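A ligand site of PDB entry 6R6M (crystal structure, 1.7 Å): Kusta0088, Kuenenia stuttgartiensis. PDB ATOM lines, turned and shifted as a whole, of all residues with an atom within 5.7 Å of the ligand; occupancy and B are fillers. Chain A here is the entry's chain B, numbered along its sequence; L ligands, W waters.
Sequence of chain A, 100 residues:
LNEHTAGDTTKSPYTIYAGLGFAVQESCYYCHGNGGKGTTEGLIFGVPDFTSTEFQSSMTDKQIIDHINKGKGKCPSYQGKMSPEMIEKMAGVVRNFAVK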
ATOM      1  N   ILE A  16      24.605   9.860  17.845  1.00  0.00           N
ATOM      2  CA  ILE A  16      24.159   9.899  16.454  1.00  0.00           C
ATOM      3  C   ILE A  16      22.662   9.622  16.357  1.00  0.00           C
ATOM      4  O   ILE A  16      21.938  10.321  15.630  1.00  0.00           O
ATOM      5  CB  ILE A  16      24.984   8.901  15.613  1.00  0.00           C
ATOM      6  CG1 ILE A  16      26.480   9.275  15.649  1.00  0.00           C
ATOM      7  CG2 ILE A  16      24.455   8.825  14.169  1.00  0.00           C
ATOM      8  CD1 ILE A  16      26.787  10.644  15.135  1.00  0.00           C
ATOM      9  N   TYR A  17      22.185   8.614  17.088  1.00  0.00           N
ATOM     10  CA  TYR A  17      20.753   8.312  17.130  1.00  0.00           C
ATOM     11  C   TYR A  17      19.955   9.528  17.586  1.00  0.00           C
ATOM     12  O   TYR A  17      18.855   9.788  17.090  1.00  0.00           O
ATOM     13  CB  TYR A  17      20.515   7.131  18.081  1.00  0.00           C
ATOM     14  CG  TYR A  17      19.193   6.388  17.960  1.00  0.00           C
ATOM     15  CD1 TYR A  17      18.020   6.907  18.529  1.00  0.00           C
ATOM     16  CD2 TYR A  17      19.133   5.153  17.351  1.00  0.00           C
ATOM     17  CE1 TYR A  17      16.817   6.183  18.457  1.00  0.00           C
ATOM     18  CE2 TYR A  17      17.945   4.435  17.274  1.00  0.00           C
ATOM     19  CZ  TYR A  17      16.788   4.967  17.829  1.00  0.00           C
ATOM     20  OH  TYR A  17      15.621   4.244  17.765  1.00  0.00           O
ATOM     21  N   VAL A  24      16.846  17.318  12.104  1.00  0.00           N
ATOM     22  CA  VAL A  24      15.875  16.614  12.934  1.00  0.00           C
ATOM     23  C   VAL A  24      15.192  15.501  12.134  1.00  0.00           C
ATOM     24  O   VAL A  24      15.110  14.354  12.574  1.00  0.00           O
ATOM     25  CB  VAL A  24      14.847  17.594  13.518  1.00  0.00           C
ATOM     26  CG1 VAL A  24      13.764  16.845  14.273  1.00  0.00           C
ATOM     27  CG2 VAL A  24      15.534  18.608  14.433  1.00  0.00           C
ATOM     28  N   GLN A  25      14.722  15.835  10.935  1.00  0.00           N
ATOM     29  CA  GLN A  25      13.987  14.856  10.128  1.00  0.00           C
ATOM     30  C   GLN A  25      14.864  13.729   9.589  1.00  0.00           C
ATOM     31  O   GLN A  25      14.336  12.784   9.000  1.00  0.00           O
ATOM     32  CB  GLN A  25      13.275  15.548   8.966  1.00  0.00           C
ATOM     33  CG  GLN A  25      14.210  16.160   7.947  1.00  0.00           C
ATOM     34  CD  GLN A  25      14.482  17.631   8.190  1.00  0.00           C
ATOM     35  OE1 GLN A  25      14.257  18.148   9.293  1.00  0.00           O
ATOM     36  NE2 GLN A  25      14.962  18.326   7.163  1.00  0.00           N
ATOM     37  N   GLU A  26      16.188  13.798   9.753  1.00  0.00           N
ATOM     38  CA  GLU A  26      17.076  12.708   9.389  1.00  0.00           C
ATOM     39  C   GLU A  26      17.732  12.055  10.593  1.00  0.00           C
ATOM     40  O   GLU A  26      18.728  11.346  10.453  1.00  0.00           O
ATOM     41  CB  GLU A  26      18.146  13.203   8.419  1.00  0.00           C
ATOM     42  CG  GLU A  26      17.702  13.204   6.965  1.00  0.00           C
ATOM     43  CD  GLU A  26      18.848  12.935   6.019  1.00  0.00           C
ATOM     44  OE1 GLU A  26      18.588  12.601   4.844  1.00  0.00           O
ATOM     45  OE2 GLU A  26      20.016  13.072   6.443  1.00  0.00           O
ATOM     46  N   SER A  27      17.192  12.295  11.787  1.00  0.00           N
ATOM     47  CA  SER A  27      17.742  11.778  13.033  1.00  0.00           C
ATOM     48  C   SER A  27      16.880  10.621  13.507  1.00  0.00           C
ATOM     49  O   SER A  27      15.656  10.761  13.571  1.00  0.00           O
ATOM     50  CB  SER A  27      17.796  12.863  14.109  1.00  0.00           C
ATOM     51  OG  SER A  27      18.406  14.062  13.636  1.00  0.00           O
ATOM     52  N   CYS A  28      17.518   9.492  13.856  1.00  0.00           N
ATOM     53  CA  CYS A  28      16.741   8.285  14.185  1.00  0.00           C
ATOM     54  C   CYS A  28      15.680   8.554  15.242  1.00  0.00           C
ATOM     55  O   CYS A  28      14.527   8.110  15.111  1.00  0.00           O
ATOM     56  CB  CYS A  28      17.642   7.141  14.700  1.00  0.00           C
ATOM     57  SG  CYS A  28      19.209   6.783  13.903  1.00  0.00           S
ATOM     58  N   TYR A  30      13.879  10.921  15.865  1.00  0.00           N
ATOM     59  CA  TYR A  30      12.701  11.663  15.439  1.00  0.00           C
ATOM     60  C   TYR A  30      11.568  10.712  15.040  1.00  0.00           C
ATOM     61  O   TYR A  30      10.395  11.008  15.259  1.00  0.00           O
ATOM     62  CB  TYR A  30      13.076  12.589  14.282  1.00  0.00           C
ATOM     63  CG  TYR A  30      11.922  13.386  13.704  1.00  0.00           C
ATOM     64  CD1 TYR A  30      11.314  14.402  14.430  1.00  0.00           C
ATOM     65  CD2 TYR A  30      11.455  13.106  12.423  1.00  0.00           C
ATOM     66  CE1 TYR A  30      10.257  15.127  13.896  1.00  0.00           C
ATOM     67  CE2 TYR A  30      10.391  13.827  11.884  1.00  0.00           C
ATOM     68  CZ  TYR A  30       9.809  14.833  12.619  1.00  0.00           C
ATOM     69  OH  TYR A  30       8.751  15.552  12.092  1.00  0.00           O
ATOM     70  N   CYS A  31      11.928   9.573  14.449  1.00  0.00           N
ATOM     71  CA  CYS A  31      10.972   8.571  13.988  1.00  0.00           C
ATOM     72  C   CYS A  31      10.948   7.338  14.868  1.00  0.00           C
ATOM     73  O   CYS A  31       9.892   6.744  15.068  1.00  0.00           O
ATOM     74  CB  CYS A  31      11.300   8.130  12.556  1.00  0.00           C
ATOM     75  SG  CYS A  31      11.348   9.450  11.277  1.00  0.00           S
ATOM     76  N   HIS A  32      12.119   6.933  15.391  1.00  0.00           N
ATOM     77  CA  HIS A  32      12.281   5.731  16.205  1.00  0.00           C
ATOM     78  C   HIS A  32      12.496   6.066  17.678  1.00  0.00           C
ATOM     79  O   HIS A  32      13.081   5.258  18.419  1.00  0.00           O
ATOM     80  CB  HIS A  32      13.443   4.883  15.684  1.00  0.00           C
ATOM     81  CG  HIS A  32      13.321   4.435  14.257  1.00  0.00           C
ATOM     82  ND1 HIS A  32      12.404   3.500  13.838  1.00  0.00           N
ATOM     83  CD2 HIS A  32      14.046   4.764  13.159  1.00  0.00           C
ATOM     84  CE1 HIS A  32      12.548   3.276  12.541  1.00  0.00           C
ATOM     85  NE2 HIS A  32      13.544   4.043  12.108  1.00  0.00           N
ATOM     86  N   GLY A  42       6.977   9.075  13.556  1.00  0.00           N
ATOM     87  CA  GLY A  42       7.413   7.792  13.022  1.00  0.00           C
ATOM     88  C   GLY A  42       6.257   6.850  12.738  1.00  0.00           C
ATOM     89  O   GLY A  42       6.259   6.139  11.720  1.00  0.00           O
ATOM     90  N   PHE A  45       4.557   7.412   9.538  1.00  0.00           N
ATOM     91  CA  PHE A  45       5.345   6.844   8.460  1.00  0.00           C
ATOM     92  C   PHE A  45       5.402   5.322   8.513  1.00  0.00           C
ATOM     93  O   PHE A  45       5.966   4.705   7.603  1.00  0.00           O
ATOM     94  CB  PHE A  45       6.759   7.418   8.492  1.00  0.00           C
ATOM     95  CG  PHE A  45       6.804   8.899   8.265  1.00  0.00           C
ATOM     96  CD1 PHE A  45       5.795   9.535   7.557  1.00  0.00           C
ATOM     97  CD2 PHE A  45       7.851   9.662   8.750  1.00  0.00           C
ATOM     98  CE1 PHE A  45       5.830  10.903   7.346  1.00  0.00           C
ATOM     99  CE2 PHE A  45       7.898  11.022   8.547  1.00  0.00           C
ATOM    100  CZ  PHE A  45       6.881  11.647   7.842  1.00  0.00           C
ATOM    101  N   GLY A  46       4.836   4.699   9.538  1.00  0.00           N
ATOM    102  CA  GLY A  46       4.807   3.256   9.582  1.00  0.00           C
ATOM    103  C   GLY A  46       6.061   2.601  10.130  1.00  0.00           C
ATOM    104  O   GLY A  46       6.406   1.495   9.679  1.00  0.00           O
ATOM    105  N   VAL A  47       6.756   3.235  11.075  1.00  0.00           N
ATOM    106  CA  VAL A  47       7.946   2.615  11.661  1.00  0.00           C
ATOM    107  C   VAL A  47       7.566   1.312  12.363  1.00  0.00           C
ATOM    108  O   VAL A  47       6.455   1.220  12.918  1.00  0.00           O
ATOM    109  CB  VAL A  47       8.668   3.538  12.661  1.00  0.00           C
ATOM    110  CG1 VAL A  47       9.235   4.785  11.963  1.00  0.00           C
ATOM    111  CG2 VAL A  47       7.777   3.906  13.838  1.00  0.00           C
ATOM    112  N   PRO A  48       8.447   0.324  12.385  1.00  0.00           N
ATOM    113  CA  PRO A  48       8.217  -0.864  13.221  1.00  0.00           C
ATOM    114  C   PRO A  48       8.502  -0.545  14.689  1.00  0.00           C
ATOM    115  O   PRO A  48       8.891   0.561  15.048  1.00  0.00           O
ATOM    116  CB  PRO A  48       9.226  -1.870  12.664  1.00  0.00           C
ATOM    117  CG  PRO A  48      10.346  -1.024  12.186  1.00  0.00           C
ATOM    118  CD  PRO A  48       9.707   0.230  11.623  1.00  0.00           C
ATOM    119  N   PHE A  50      10.880  -1.487  17.540  1.00  0.00           N
ATOM    120  CA  PHE A  50      12.162  -2.103  17.853  1.00  0.00           C
ATOM    121  C   PHE A  50      12.129  -2.891  19.167  1.00  0.00           C
ATOM    122  O   PHE A  50      13.000  -3.743  19.385  1.00  0.00           O
ATOM    123  CB  PHE A  50      13.284  -1.050  17.959  1.00  0.00           C
ATOM    124  CG  PHE A  50      13.657  -0.360  16.649  1.00  0.00           C
ATOM    125  CD1 PHE A  50      13.322  -0.889  15.403  1.00  0.00           C
ATOM    126  CD2 PHE A  50      14.391   0.832  16.686  1.00  0.00           C
ATOM    127  CE1 PHE A  50      13.699  -0.216  14.214  1.00  0.00           C
ATOM    128  CE2 PHE A  50      14.765   1.502  15.522  1.00  0.00           C
ATOM    129  CZ  PHE A  50      14.428   0.969  14.300  1.00  0.00           C
ATOM    130  N   PHE A  55       9.224  -8.072  15.569  1.00  0.00           N
ATOM    131  CA  PHE A  55      10.003  -7.332  14.591  1.00  0.00           C
ATOM    132  C   PHE A  55      11.444  -7.820  14.551  1.00  0.00           C
ATOM    133  O   PHE A  55      12.007  -8.031  13.470  1.00  0.00           O
ATOM    134  CB  PHE A  55       9.981  -5.830  14.899  1.00  0.00           C
ATOM    135  CG  PHE A  55      11.157  -5.095  14.311  1.00  0.00           C
ATOM    136  CD1 PHE A  55      11.169  -4.746  12.966  1.00  0.00           C
ATOM    137  CD2 PHE A  55      12.282  -4.829  15.073  1.00  0.00           C
ATOM    138  CE1 PHE A  55      12.257  -4.092  12.414  1.00  0.00           C
ATOM    139  CE2 PHE A  55      13.370  -4.174  14.520  1.00  0.00           C
ATOM    140  CZ  PHE A  55      13.354  -3.803  13.193  1.00  0.00           C
ATOM    141  N   MET A  59      14.433  -9.683  10.962  1.00  0.00           N
ATOM    142  CA  MET A  59      15.667  -9.226  10.328  1.00  0.00           C
ATOM    143  C   MET A  59      16.853  -9.964  10.926  1.00  0.00           C
ATOM    144  O   MET A  59      16.889 -10.220  12.130  1.00  0.00           O
ATOM    145  CB  MET A  59      15.875  -7.714  10.529  1.00  0.00           C
ATOM    146  CG  MET A  59      14.760  -6.874   9.957  1.00  0.00           C
ATOM    147  SD  MET A  59      15.086  -5.106  10.101  1.00  0.00           S
ATOM    148  CE  MET A  59      16.301  -4.893   8.790  1.00  0.00           C
ATOM    149  N   ILE A  64      20.045  -5.703   9.086  1.00  0.00           N
ATOM    150  CA  ILE A  64      19.963  -4.409   9.757  1.00  0.00           C
ATOM    151  C   ILE A  64      21.070  -3.487   9.252  1.00  0.00           C
ATOM    152  O   ILE A  64      20.825  -2.311   8.940  1.00  0.00           O
ATOM    153  CB  ILE A  64      20.003  -4.572  11.285  1.00  0.00           C
ATOM    154  CG1 ILE A  64      18.736  -5.302  11.766  1.00  0.00           C
ATOM    155  CG2 ILE A  64      20.056  -3.199  11.954  1.00  0.00           C
ATOM    156  CD1 ILE A  64      18.756  -5.640  13.264  1.00  0.00           C
ATOM    157  N   HIS A  67      20.282  -2.415   5.778  1.00  0.00           N
ATOM    158  CA  HIS A  67      19.183  -1.460   5.773  1.00  0.00           C
ATOM    159  C   HIS A  67      19.674  -0.075   6.134  1.00  0.00           C
ATOM    160  O   HIS A  67      19.310   0.903   5.478  1.00  0.00           O
ATOM    161  CB  HIS A  67      18.084  -1.861   6.757  1.00  0.00           C
ATOM    162  CG  HIS A  67      17.062  -0.778   6.914  1.00  0.00           C
ATOM    163  ND1 HIS A  67      16.020  -0.604   6.027  1.00  0.00           N
ATOM    164  CD2 HIS A  67      16.973   0.225   7.820  1.00  0.00           C
ATOM    165  CE1 HIS A  67      15.315   0.449   6.385  1.00  0.00           C
ATOM    166  NE2 HIS A  67      15.869   0.979   7.473  1.00  0.00           N
ATOM    167  N   ILE A  68      20.470   0.040   7.214  1.00  0.00           N
ATOM    168  CA  ILE A  68      20.958   1.354   7.619  1.00  0.00           C
ATOM    169  C   ILE A  68      21.761   1.992   6.493  1.00  0.00           C
ATOM    170  O   ILE A  68      21.663   3.194   6.243  1.00  0.00           O
ATOM    171  CB  ILE A  68      21.747   1.266   8.935  1.00  0.00           C
ATOM    172  CG1 ILE A  68      20.803   0.921  10.094  1.00  0.00           C
ATOM    173  CG2 ILE A  68      22.508   2.579   9.203  1.00  0.00           C
ATOM    174  CD1 ILE A  68      21.495   0.409  11.354  1.00  0.00           C
ATOM    175  N   LYS A  72      15.142   2.692   3.270  1.00  0.00           N
ATOM    176  CA  LYS A  72      13.985   2.126   2.579  1.00  0.00           C
ATOM    177  C   LYS A  72      12.831   3.088   2.753  1.00  0.00           C
ATOM    178  O   LYS A  72      12.389   3.332   3.869  1.00  0.00           O
ATOM    179  CB  LYS A  72      13.625   0.739   3.123  1.00  0.00           C
ATOM    180  CG  LYS A  72      12.508   0.059   2.345  1.00  0.00           C
ATOM    181  CD  LYS A  72      12.198  -1.341   2.871  1.00  0.00           C
ATOM    182  CE  LYS A  72      11.266  -2.049   1.874  1.00  0.00           C
ATOM    183  NZ  LYS A  72      10.873  -3.401   2.320  1.00  0.00           N
ATOM    184  N   GLY A  73      12.358   3.642   1.651  1.00  0.00           N
ATOM    185  CA  GLY A  73      11.219   4.545   1.743  1.00  0.00           C
ATOM    186  C   GLY A  73      11.554   5.770   2.552  1.00  0.00           C
ATOM    187  O   GLY A  73      12.521   6.494   2.268  1.00  0.00           O
ATOM    188  N   LYS A  74      10.776   6.019   3.607  1.00  0.00           N
ATOM    189  CA  LYS A  74      11.009   7.205   4.418  1.00  0.00           C
ATOM    190  C   LYS A  74      12.134   7.026   5.424  1.00  0.00           C
ATOM    191  O   LYS A  74      12.574   8.025   6.008  1.00  0.00           O
ATOM    192  CB  LYS A  74       9.724   7.625   5.125  1.00  0.00           C
ATOM    193  CG  LYS A  74       8.641   7.969   4.130  1.00  0.00           C
ATOM    194  CD  LYS A  74       7.636   8.936   4.677  1.00  0.00           C
ATOM    195  CE  LYS A  74       7.015   9.713   3.527  1.00  0.00           C
ATOM    196  NZ  LYS A  74       6.808   8.820   2.345  1.00  0.00           N
ATOM    197  N   CYS A  75      12.618   5.797   5.613  1.00  0.00           N
ATOM    198  CA  CYS A  75      13.828   5.594   6.416  1.00  0.00           C
ATOM    199  C   CYS A  75      15.029   5.979   5.571  1.00  0.00           C
ATOM    200  O   CYS A  75      15.283   5.364   4.530  1.00  0.00           O
ATOM    201  CB  CYS A  75      13.966   4.151   6.888  1.00  0.00           C
ATOM    202  SG  CYS A  75      15.302   3.956   8.092  1.00  0.00           S
ATOM    203  N   PRO A  76      15.778   7.006   5.967  1.00  0.00           N
ATOM    204  CA  PRO A  76      16.855   7.503   5.097  1.00  0.00           C
ATOM    205  C   PRO A  76      18.005   6.524   4.963  1.00  0.00           C
ATOM    206  O   PRO A  76      18.235   5.656   5.813  1.00  0.00           O
ATOM    207  CB  PRO A  76      17.314   8.803   5.775  1.00  0.00           C
ATOM    208  CG  PRO A  76      16.209   9.189   6.700  1.00  0.00           C
ATOM    209  CD  PRO A  76      15.563   7.869   7.137  1.00  0.00           C
ATOM    210  N   TYR A  78      21.935   5.924   5.210  1.00  0.00           N
ATOM    211  CA  TYR A  78      23.002   6.525   5.988  1.00  0.00           C
ATOM    212  C   TYR A  78      24.400   6.139   5.512  1.00  0.00           C
ATOM    213  O   TYR A  78      25.377   6.553   6.140  1.00  0.00           O
ATOM    214  CB  TYR A  78      22.815   6.168   7.478  1.00  0.00           C
ATOM    215  CG  TYR A  78      21.638   6.893   8.046  1.00  0.00           C
ATOM    216  CD1 TYR A  78      20.338   6.349   7.950  1.00  0.00           C
ATOM    217  CD2 TYR A  78      21.781   8.150   8.620  1.00  0.00           C
ATOM    218  CE1 TYR A  78      19.237   7.051   8.439  1.00  0.00           C
ATOM    219  CE2 TYR A  78      20.686   8.845   9.105  1.00  0.00           C
ATOM    220  CZ  TYR A  78      19.429   8.298   9.012  1.00  0.00           C
ATOM    221  OH  TYR A  78      18.356   9.007   9.513  1.00  0.00           O
ATOM    222  N   MET A  82      27.666   8.035   8.222  1.00  0.00           N
ATOM    223  CA  MET A  82      28.452   7.587   9.363  1.00  0.00           C
ATOM    224  C   MET A  82      29.344   6.449   8.885  1.00  0.00           C
ATOM    225  O   MET A  82      29.120   5.875   7.808  1.00  0.00           O
ATOM    226  CB  MET A  82      27.562   7.153  10.543  1.00  0.00           C
ATOM    227  CG  MET A  82      26.504   6.130  10.199  1.00  0.00           C
ATOM    228  SD  MET A  82      25.459   5.661  11.613  1.00  0.00           S
ATOM    229  CE  MET A  82      23.908   6.338  11.066  1.00  0.00           C
ATOM    230  N   MET A  90      25.359   0.923  15.401  1.00  0.00           N
ATOM    231  CA  MET A  90      23.959   1.322  15.350  1.00  0.00           C
ATOM    232  C   MET A  90      23.052   0.103  15.231  1.00  0.00           C
ATOM    233  O   MET A  90      21.959   0.072  15.805  1.00  0.00           O
ATOM    234  CB  MET A  90      23.725   2.283  14.185  1.00  0.00           C
ATOM    235  CG  MET A  90      22.421   3.040  14.321  1.00  0.00           C
ATOM    236  SD  MET A  90      22.386   4.149  15.752  1.00  0.00           S
ATOM    237  CE  MET A  90      23.460   5.466  15.200  1.00  0.00           C
ATOM    238  N   VAL A  94      19.805  -0.908  17.641  1.00  0.00           N
ATOM    239  CA  VAL A  94      18.499  -1.413  17.206  1.00  0.00           C
ATOM    240  C   VAL A  94      18.155  -2.704  17.926  1.00  0.00           C
ATOM    241  O   VAL A  94      17.054  -2.849  18.475  1.00  0.00           O
ATOM    242  CB  VAL A  94      18.460  -1.577  15.674  1.00  0.00           C
ATOM    243  CG1 VAL A  94      17.160  -2.274  15.225  1.00  0.00           C
ATOM    244  CG2 VAL A  94      18.577  -0.226  15.017  1.00  0.00           C
HETATM  245 FE1  LIG L   1      14.244   3.948  10.286  1.00  0.00          FE
HETATM  246  C1  LIG L   1      12.583   1.145   9.299  1.00  0.00           C
HETATM  247  C2  LIG L   1      16.781   1.980  11.472  1.00  0.00           C
HETATM  248  C3  LIG L   1      16.029   6.729  11.036  1.00  0.00           C
HETATM  249  C4  LIG L   1      11.546   5.933   9.464  1.00  0.00           C
HETATM  250  N1  LIG L   1      14.612   1.981  10.341  1.00  0.00           N
HETATM  251  C5  LIG L   1      13.777   0.945   9.935  1.00  0.00           C
HETATM  252  C6  LIG L   1      14.366  -0.333  10.288  1.00  0.00           C
HETATM  253  C7  LIG L   1      15.523  -0.081  10.889  1.00  0.00           C
HETATM  254  C8  LIG L   1      15.709   1.347  10.912  1.00  0.00           C
HETATM  255  C9  LIG L   1      16.546  -1.095  11.450  1.00  0.00           C
HETATM  256  C10 LIG L   1      13.729  -1.716   9.988  1.00  0.00           C
HETATM  257  C11 LIG L   1      13.960  -2.057   8.525  1.00  0.00           C
HETATM  258  C12 LIG L   1      12.681  -1.915   7.737  1.00  0.00           C
HETATM  259  O1  LIG L   1      12.777  -1.525   6.542  1.00  0.00           O
HETATM  260  O2  LIG L   1      11.583  -2.184   8.293  1.00  0.00           O
HETATM  261  N2  LIG L   1      15.996   4.286  11.034  1.00  0.00           N
HETATM  262  C13 LIG L   1      16.934   3.342  11.482  1.00  0.00           C
HETATM  263  C14 LIG L   1      18.143   3.981  11.931  1.00  0.00           C
HETATM  264  C15 LIG L   1      17.936   5.297  11.840  1.00  0.00           C
HETATM  265  C16 LIG L   1      16.611   5.505  11.260  1.00  0.00           C
HETATM  266  C17 LIG L   1      19.362   3.211  12.530  1.00  0.00           C
HETATM  267  C18 LIG L   1      18.904   6.441  12.202  1.00  0.00           C
HETATM  268  C19 LIG L   1      20.298   6.268  11.552  1.00  0.00           C
HETATM  269  N3  LIG L   1      13.836   5.902  10.296  1.00  0.00           N
HETATM  270  C20 LIG L   1      14.739   6.917  10.609  1.00  0.00           C
HETATM  271  C21 LIG L   1      14.132   8.210  10.323  1.00  0.00           C
HETATM  272  C22 LIG L   1      12.876   7.993   9.933  1.00  0.00           C
HETATM  273  C23 LIG L   1      12.685   6.557   9.889  1.00  0.00           C
HETATM  274  C24 LIG L   1      14.835   9.539  10.638  1.00  0.00           C
HETATM  275  C25 LIG L   1      11.767   9.027   9.599  1.00  0.00           C
HETATM  276  C26 LIG L   1      12.180  10.170   8.654  1.00  0.00           C
HETATM  277  N4  LIG L   1      12.434   3.615   9.574  1.00  0.00           N
HETATM  278  C27 LIG L   1      11.484   4.591   9.226  1.00  0.00           C
HETATM  279  C28 LIG L   1      10.351   3.985   8.556  1.00  0.00           C
HETATM  280  C29 LIG L   1      10.677   2.513   8.490  1.00  0.00           C
HETATM  281  C30 LIG L   1      11.953   2.362   9.145  1.00  0.00           C
HETATM  282  C31 LIG L   1       9.117   4.693   7.992  1.00  0.00           C
HETATM  283  C32 LIG L   1       9.852   1.391   7.867  1.00  0.00           C
HETATM  284  C33 LIG L   1      10.405   1.254   6.440  1.00  0.00           C
HETATM  285  C34 LIG L   1       9.748   0.092   5.723  1.00  0.00           C
HETATM  286  O3  LIG L   1       9.247   0.301   4.594  1.00  0.00           O
HETATM  287  O4  LIG L   1       9.714  -1.035   6.286  1.00  0.00           O
HETATM  288  O   HOH W   1      15.266  -2.802   4.564  1.00  0.00           O
HETATM  289  O   HOH W   2      13.540  12.491   6.422  1.00  0.00           O
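C18 of the ligand is bonded to SG of Cys 28, 1.8 Å away. The side-chain sulfur of Cys 31 is bonded to a carbon (C25) of the ligand (1.8 Å). NE2 of His 32 is bound to FE1 of the ligand (2.0 Å). O1 of the ligand sits close to ND1 of His 67 (3.4 Å). An iron atom (FE1) of the ligand is bound by the side-chain sulfur (SG) of Cys 75 (2.4 Å).
OH of Tyr 78 lies within hydrogen-bond range of O of Glu 26, at 2.5 Å. N of Val 47 sits at hydrogen-bond distance from O of Gly 42, 3.0 Å away. The backbone NH of Tyr 78 sits at hydrogen-bond distance from the backbone carbonyl oxygen of Ile 68, 2.9 Å away. OG of Ser 27 sits close to O of Val 24 (3.5 Å). The side-chain hydroxyl (OH) of Tyr 17 is in hydrogen-bond range of the backbone carbonyl oxygen (O) of His 32, 2.8 Å away. SG of Cys 75 sits close to NE2 of His 67, 3.1 Å away.
Gln 25 touches the ligand (O to C26, 3.4 Å). Glu 26 touches the ligand (C to C24, 3.8 Å). O of Ser 27 touches C24 of the ligand, at 3.3 Å. O of Phe 45 touches C31 of the ligand (3.2 Å). Gly 46 touches the ligand. Val 47 touches the ligand. Pro 48 touches the ligand. Phe 50 touches the ligand (CZ to C8, 3.6 Å). Phe 55 touches the ligand. Met 59 touches the ligand. CG1 of Ile 68 touches C17 of the ligand (3.6 Å). Lys 72 touches the ligand (CD to O1, 3.7 Å). O of Lys 74 touches C26 of the ligand, at 3.4 Å. Pro 76 touches the ligand. CZ of Tyr 78 touches C19 of the ligand, at 3.4 Å. Met 82 touches the ligand (CE to C19, 3.6 Å). CG of Met 90 touches C17 of the ligand (3.5 Å). Hydrophobic or aromatic side chains that line the ligand: His 32, Phe 45, Val 47, Pro 48, Phe 50, Phe 55, Met 59, His 67, Ile 68, Pro 76, Tyr 78, Met 82 and Met 90. Within 4 Å of the ligand: Gln 25, Glu 26, Ser 27, Cys 28, Cys 31, His 32, Phe 45, Gly 46, Val 47, Pro 48, Phe 50, Phe 55, Met 59, His 67, Ile 68, Lys 72, Lys 74, Cys 75, Pro 76, Tyr 78, Met 82 and Met 90. The nearest printed residue that does not touch the ligand is Val 94 (4.002 Å).
Water W1 bridges a ring nitrogen (ND1) of His 67 (2.7 Å) and an oxygen (O1) of the ligand (3.4 Å).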
